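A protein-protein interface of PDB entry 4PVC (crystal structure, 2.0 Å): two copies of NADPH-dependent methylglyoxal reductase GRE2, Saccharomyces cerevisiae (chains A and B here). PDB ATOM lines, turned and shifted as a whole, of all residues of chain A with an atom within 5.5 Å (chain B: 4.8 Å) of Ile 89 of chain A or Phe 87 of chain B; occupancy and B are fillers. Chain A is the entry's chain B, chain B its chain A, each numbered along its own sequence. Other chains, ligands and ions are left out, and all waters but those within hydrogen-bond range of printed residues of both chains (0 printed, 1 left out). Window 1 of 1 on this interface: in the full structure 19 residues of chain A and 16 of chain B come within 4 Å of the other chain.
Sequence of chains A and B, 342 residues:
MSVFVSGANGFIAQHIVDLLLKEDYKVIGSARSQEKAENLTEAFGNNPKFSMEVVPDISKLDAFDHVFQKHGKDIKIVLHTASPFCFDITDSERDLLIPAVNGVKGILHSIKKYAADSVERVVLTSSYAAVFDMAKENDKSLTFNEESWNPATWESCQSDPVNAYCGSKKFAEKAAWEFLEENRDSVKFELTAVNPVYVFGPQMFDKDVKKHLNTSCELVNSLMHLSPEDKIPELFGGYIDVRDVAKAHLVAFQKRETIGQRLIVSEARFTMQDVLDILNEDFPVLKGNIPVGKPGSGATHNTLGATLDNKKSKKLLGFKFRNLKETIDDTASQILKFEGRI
Of the printed residues of chain B, Phe 85 of chain A touches Asp 88.
Of the printed residues of chain B, Cys 86 of chain A touches Cys 86 and Phe 87.
Printed residues of chain B within 4 Å of Phe 87 of chain A: Cys 86 and Phe 87.
Of chain B, only Phe 87 comes within 4 Å of Ile 89 of chain A.
Phe 85 of chain B touches none of the printed residues of chain A.
Of the printed residues of chain A, Cys 86 of chain B touches Cys 86 (3.2 Å), Phe 87 (3.3 Å) and Asp 88 (3.9 Å).
Phe 87 of chain B touches just these residues of chain A: Cys 86, Phe 87, Asp 88 and Ile 89.
Of the printed residues of chain A, Asp 88 of chain B touches Phe 85.
Thr 215 of chain B touches none of the printed residues of chain A.
The nearest printed residue of chain B that does not touch Ile 89 of chain A is Thr 215 of chain B (4.8 Å).
Phe 85 of chain A touches Asp 88 of chain B, but with the chains exchanged Asp 88 of chain A does not touch Phe 85 of chain B (4.3 Å).
Cys 86 of chain B touches its own counterpart, Cys 86 of chain A.
Cys 86 of chain A touches Phe 87 of chain B, and with the chains exchanged Phe 87 of chain A touches Cys 86 of chain B.
Ile 89 of chain A touches Phe 87 of chain B, but with the chains exchanged Phe 87 of chain A does not touch Ile 89 of chain B (4.2 Å).
Positions printed for both chains: 85, 86, 87, 88 and 89.
Of the 8 pairs that touch across the chains among the printed residues, 4 have their exchanged pair printed and touching as well.
Phe 85 of chain A touches Asp 88 of chain B.
Cys 86 of chain A touches Phe 87 of chain B (CA to O, 3.5 Å).
Cys 86 of chain B touches Phe 87 of chain A (CA to O, 3.3 Å).
Asp 88 of chain A touches Cys 86 of chain B (OD1 to N, 3.9 Å).
OD1 of Asp 88 of chain A touches CD1 of Phe 87 of chain B, at 3.6 Å.
Ile 89 of chain A touches Phe 87 of chain B (CG2 to CE1, 3.9 Å).
The backbone NH (N) of Thr 90 of chain A is in hydrogen-bond range of the side-chain carboxylate (OD2) of Asp 88 of chain A (3.4 Å).
The backbone carbonyl oxygen of Ile 89 of chain A sits at hydrogen-bond distance from the side-chain hydroxyl of Ser 92 of chain A.
SG of Cys 86 of chain B lies close to SG of Cys 86 of chain A, at 3.5 Å.
The backbone NH (N) of Phe 87 of chain B is in hydrogen-bond range of the backbone carbonyl oxygen (O) of Phe 87 of chain A (2.7 Å).
Of the 8 printed residues of chain B, 3 touch a printed residue of chain A.
Hydrophobic or aromatic side chains of chain B within 4 Å of the printed part of chain A: Phe 87.
Hydrophobic or aromatic side chains of chain A within 4 Å of the printed part of chain B: Phe 87 and Ile 89.
Among the printed residues, no Asp or Glu carboxylate lies within 4 Å of a Lys or Arg side-chain nitrogen of the other chain.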
ATOM      1  N   PHE A  85      -1.938 -15.909 -15.323  1.00  0.00           N
ATOM      2  CA  PHE A  85      -1.667 -16.878 -14.246  1.00  0.00           C
ATOM      3  C   PHE A  85      -2.867 -17.700 -13.770  1.00  0.00           C
ATOM      4  O   PHE A  85      -2.699 -18.797 -13.234  1.00  0.00           O
ATOM      5  CB  PHE A  85      -0.927 -16.227 -13.063  1.00  0.00           C
ATOM      6  CG  PHE A  85      -1.789 -15.353 -12.179  1.00  0.00           C
ATOM      7  CD1 PHE A  85      -1.838 -13.974 -12.380  1.00  0.00           C
ATOM      8  CD2 PHE A  85      -2.516 -15.903 -11.123  1.00  0.00           C
ATOM      9  CE1 PHE A  85      -2.616 -13.159 -11.558  1.00  0.00           C
ATOM     10  CE2 PHE A  85      -3.296 -15.097 -10.296  1.00  0.00           C
ATOM     11  CZ  PHE A  85      -3.348 -13.724 -10.514  1.00  0.00           C
ATOM     12  N   CYS A  86      -4.069 -17.171 -13.968  1.00  0.00           N
ATOM     13  CA  CYS A  86      -5.286 -17.906 -13.640  1.00  0.00           C
ATOM     14  C   CYS A  86      -6.466 -17.423 -14.478  1.00  0.00           C
ATOM     15  O   CYS A  86      -6.396 -16.366 -15.113  1.00  0.00           O
ATOM     16  CB  CYS A  86      -5.600 -17.777 -12.149  1.00  0.00           C
ATOM     17  SG  CYS A  86      -6.260 -16.168 -11.664  1.00  0.00           S
ATOM     18  N   PHE A  87      -7.539 -18.204 -14.464  1.00  0.00           N
ATOM     19  CA  PHE A  87      -8.750 -17.932 -15.214  1.00  0.00           C
ATOM     20  C   PHE A  87      -9.994 -18.591 -14.626  1.00  0.00           C
ATOM     21  O   PHE A  87      -9.900 -19.414 -13.748  1.00  0.00           O
ATOM     22  CB  PHE A  87      -8.595 -18.421 -16.631  1.00  0.00           C
ATOM     23  CG  PHE A  87      -8.674 -19.911 -16.774  1.00  0.00           C
ATOM     24  CD1 PHE A  87      -9.871 -20.527 -17.053  1.00  0.00           C
ATOM     25  CD2 PHE A  87      -7.536 -20.694 -16.636  1.00  0.00           C
ATOM     26  CE1 PHE A  87      -9.945 -21.883 -17.187  1.00  0.00           C
ATOM     27  CE2 PHE A  87      -7.597 -22.073 -16.767  1.00  0.00           C
ATOM     28  CZ  PHE A  87      -8.779 -22.666 -17.051  1.00  0.00           C
ATOM     29  N   ASP A  88     -11.167 -18.199 -15.115  1.00  0.00           N
ATOM     30  CA  ASP A  88     -12.399 -18.907 -14.763  1.00  0.00           C
ATOM     31  C   ASP A  88     -13.354 -19.076 -15.946  1.00  0.00           C
ATOM     32  O   ASP A  88     -13.211 -18.415 -16.981  1.00  0.00           O
ATOM     33  CB  ASP A  88     -13.114 -18.259 -13.574  1.00  0.00           C
ATOM     34  CG  ASP A  88     -14.038 -19.237 -12.855  1.00  0.00           C
ATOM     35  OD1 ASP A  88     -13.531 -20.208 -12.240  1.00  0.00           O
ATOM     36  OD2 ASP A  88     -15.273 -19.036 -12.910  1.00  0.00           O
ATOM     37  N   ILE A  89     -14.331 -19.963 -15.762  1.00  0.00           N
ATOM     38  CA  ILE A  89     -15.206 -20.437 -16.836  1.00  0.00           C
ATOM     39  C   ILE A  89     -16.513 -19.645 -16.985  1.00  0.00           C
ATOM     40  O   ILE A  89     -17.122 -19.642 -18.059  1.00  0.00           O
ATOM     41  CB  ILE A  89     -15.498 -21.954 -16.682  1.00  0.00           C
ATOM     42  CG1 ILE A  89     -16.186 -22.253 -15.341  1.00  0.00           C
ATOM     43  CG2 ILE A  89     -14.199 -22.753 -16.822  1.00  0.00           C
ATOM     44  CD1 ILE A  89     -16.722 -23.675 -15.200  1.00  0.00           C
ATOM     45  N   THR A  90     -16.942 -18.990 -15.909  1.00  0.00           N
ATOM     46  CA  THR A  90     -18.091 -18.087 -15.960  1.00  0.00           C
ATOM     47  C   THR A  90     -17.582 -16.677 -16.255  1.00  0.00           C
ATOM     48  O   THR A  90     -16.579 -16.242 -15.680  1.00  0.00           O
ATOM     49  CB  THR A  90     -18.906 -18.110 -14.650  1.00  0.00           C
ATOM     50  OG1 THR A  90     -19.128 -19.467 -14.250  1.00  0.00           O
ATOM     51  CG2 THR A  90     -20.256 -17.415 -14.829  1.00  0.00           C
ATOM     52  N   ASP A  91     -18.289 -15.977 -17.142  1.00  0.00           N
ATOM     53  CA  ASP A  91     -17.819 -14.722 -17.740  1.00  0.00           C
ATOM     54  C   ASP A  91     -16.448 -14.952 -18.384  1.00  0.00           C
ATOM     55  O   ASP A  91     -15.436 -14.378 -17.966  1.00  0.00           O
ATOM     56  CB  ASP A  91     -17.800 -13.569 -16.721  1.00  0.00           C
ATOM     57  CG  ASP A  91     -17.813 -12.187 -17.380  1.00  0.00           C
ATOM     58  OD1 ASP A  91     -17.590 -12.084 -18.608  1.00  0.00           O
ATOM     59  OD2 ASP A  91     -18.042 -11.191 -16.658  1.00  0.00           O
ATOM     60  N   SER A  92     -16.443 -15.821 -19.395  1.00  0.00           N
ATOM     61  CA  SER A  92     -15.247 -16.160 -20.171  1.00  0.00           C
ATOM     62  C   SER A  92     -14.542 -14.917 -20.695  1.00  0.00           C
ATOM     63  O   SER A  92     -13.317 -14.833 -20.672  1.00  0.00           O
ATOM     64  CB  SER A  92     -15.611 -17.059 -21.357  1.00  0.00           C
ATOM     65  OG  SER A  92     -16.407 -18.156 -20.953  1.00  0.00           O
ATOM     66  N   PRO A 161     -16.027 -24.225 -21.763  1.00  0.00           N
ATOM     67  CA  PRO A 161     -14.686 -23.864 -21.283  1.00  0.00           C
ATOM     68  C   PRO A 161     -13.547 -24.223 -22.239  1.00  0.00           C
ATOM     69  O   PRO A 161     -12.651 -23.403 -22.455  1.00  0.00           O
ATOM     70  CB  PRO A 161     -14.554 -24.666 -19.986  1.00  0.00           C
ATOM     71  CG  PRO A 161     -15.959 -24.817 -19.507  1.00  0.00           C
ATOM     72  CD  PRO A 161     -16.772 -24.997 -20.749  1.00  0.00           C
ATOM     73  N   PHE B  85     -12.626 -18.367  -6.889  1.00  0.00           N
ATOM     74  CA  PHE B  85     -12.575 -17.694  -8.154  1.00  0.00           C
ATOM     75  C   PHE B  85     -11.193 -17.849  -8.681  1.00  0.00           C
ATOM     76  O   PHE B  85     -10.238 -17.702  -7.982  1.00  0.00           O
ATOM     77  CB  PHE B  85     -12.873 -16.234  -8.011  1.00  0.00           C
ATOM     78  CG  PHE B  85     -12.793 -15.494  -9.290  1.00  0.00           C
ATOM     79  CD1 PHE B  85     -11.632 -14.850  -9.652  1.00  0.00           C
ATOM     80  CD2 PHE B  85     -13.885 -15.410 -10.122  1.00  0.00           C
ATOM     81  CE1 PHE B  85     -11.547 -14.139 -10.820  1.00  0.00           C
ATOM     82  CE2 PHE B  85     -13.820 -14.717 -11.289  1.00  0.00           C
ATOM     83  CZ  PHE B  85     -12.627 -14.075 -11.639  1.00  0.00           C
ATOM     84  N   CYS B  86     -11.125 -18.195  -9.929  1.00  0.00           N
ATOM     85  CA  CYS B  86      -9.887 -18.392 -10.661  1.00  0.00           C
ATOM     86  C   CYS B  86      -9.518 -19.802 -10.498  1.00  0.00           C
ATOM     87  O   CYS B  86      -9.843 -20.402  -9.521  1.00  0.00           O
ATOM     88  CB  CYS B  86      -8.689 -17.639 -10.113  1.00  0.00           C
ATOM     89  SG  CYS B  86      -7.393 -18.877  -9.700  1.00  0.00           S
ATOM     90  N   PHE B  87      -8.760 -20.304 -11.430  1.00  0.00           N
ATOM     91  CA  PHE B  87      -8.128 -21.557 -11.232  1.00  0.00           C
ATOM     92  C   PHE B  87      -7.032 -21.735 -12.242  1.00  0.00           C
ATOM     93  O   PHE B  87      -6.921 -20.954 -13.148  1.00  0.00           O
ATOM     94  CB  PHE B  87      -9.120 -22.701 -11.187  1.00  0.00           C
ATOM     95  CG  PHE B  87      -9.679 -23.087 -12.497  1.00  0.00           C
ATOM     96  CD1 PHE B  87     -10.768 -22.444 -13.009  1.00  0.00           C
ATOM     97  CD2 PHE B  87      -9.165 -24.146 -13.195  1.00  0.00           C
ATOM     98  CE1 PHE B  87     -11.278 -22.839 -14.185  1.00  0.00           C
ATOM     99  CE2 PHE B  87      -9.697 -24.509 -14.361  1.00  0.00           C
ATOM    100  CZ  PHE B  87     -10.728 -23.862 -14.848  1.00  0.00           C
ATOM    101  N   ASP B  88      -6.204 -22.745 -12.050  1.00  0.00           N
ATOM    102  CA  ASP B  88      -5.159 -23.046 -13.026  1.00  0.00           C
ATOM    103  C   ASP B  88      -5.030 -24.558 -13.190  1.00  0.00           C
ATOM    104  O   ASP B  88      -5.302 -25.321 -12.256  1.00  0.00           O
ATOM    105  CB  ASP B  88      -3.820 -22.428 -12.609  1.00  0.00           C
ATOM    106  CG  ASP B  88      -2.672 -22.857 -13.507  1.00  0.00           C
ATOM    107  OD1 ASP B  88      -2.610 -22.385 -14.665  1.00  0.00           O
ATOM    108  OD2 ASP B  88      -1.835 -23.672 -13.055  1.00  0.00           O
ATOM    109  N   ILE B  89      -4.603 -24.976 -14.381  1.00  0.00           N
ATOM    110  CA  ILE B  89      -4.621 -26.388 -14.774  1.00  0.00           C
ATOM    111  C   ILE B  89      -3.248 -27.081 -14.787  1.00  0.00           C
ATOM    112  O   ILE B  89      -3.170 -28.302 -14.957  1.00  0.00           O
ATOM    113  CB  ILE B  89      -5.352 -26.588 -16.133  1.00  0.00           C
ATOM    114  CG1 ILE B  89      -4.722 -25.712 -17.227  1.00  0.00           C
ATOM    115  CG2 ILE B  89      -6.844 -26.283 -15.977  1.00  0.00           C
ATOM    116  CD1 ILE B  89      -5.213 -26.003 -18.640  1.00  0.00           C
ATOM    117  N   ASP B  95      -3.514 -24.744  -7.247  1.00  0.00           N
ATOM    118  CA  ASP B  95      -4.368 -23.719  -7.858  1.00  0.00           C
ATOM    119  C   ASP B  95      -5.839 -24.099  -8.044  1.00  0.00           C
ATOM    120  O   ASP B  95      -6.637 -23.294  -8.534  1.00  0.00           O
ATOM    121  CB  ASP B  95      -3.762 -23.261  -9.189  1.00  0.00           C
ATOM    122  CG  ASP B  95      -2.359 -22.699  -9.030  1.00  0.00           C
ATOM    123  OD1 ASP B  95      -2.047 -22.166  -7.943  1.00  0.00           O
ATOM    124  OD2 ASP B  95      -1.565 -22.791  -9.990  1.00  0.00           O
ATOM    125  N   LEU B  96      -6.200 -25.319  -7.652  1.00  0.00           N
ATOM    126  CA  LEU B  96      -7.581 -25.776  -7.787  1.00  0.00           C
ATOM    127  C   LEU B  96      -8.038 -26.609  -6.587  1.00  0.00           C
ATOM    128  O   LEU B  96      -9.055 -26.297  -5.956  1.00  0.00           O
ATOM    129  CB  LEU B  96      -7.758 -26.550  -9.099  1.00  0.00           C
ATOM    130  CG  LEU B  96      -9.129 -27.121  -9.468  1.00  0.00           C
ATOM    131  CD1 LEU B  96     -10.201 -26.039  -9.570  1.00  0.00           C
ATOM    132  CD2 LEU B  96      -9.024 -27.890 -10.774  1.00  0.00           C
ATOM    133  N   THR B 215     -22.197 -21.606 -17.365  1.00  0.00           N
ATOM    134  CA  THR B 215     -21.759 -22.610 -18.343  1.00  0.00           C
ATOM    135  C   THR B 215     -22.908 -23.314 -19.078  1.00  0.00           C
ATOM    136  O   THR B 215     -22.851 -23.486 -20.300  1.00  0.00           O
ATOM    137  CB  THR B 215     -20.785 -23.657 -17.724  1.00  0.00           C
ATOM    138  OG1 THR B 215     -20.610 -24.747 -18.640  1.00  0.00           O
ATOM    139  CG2 THR B 215     -21.312 -24.206 -16.400  1.00  0.00           C
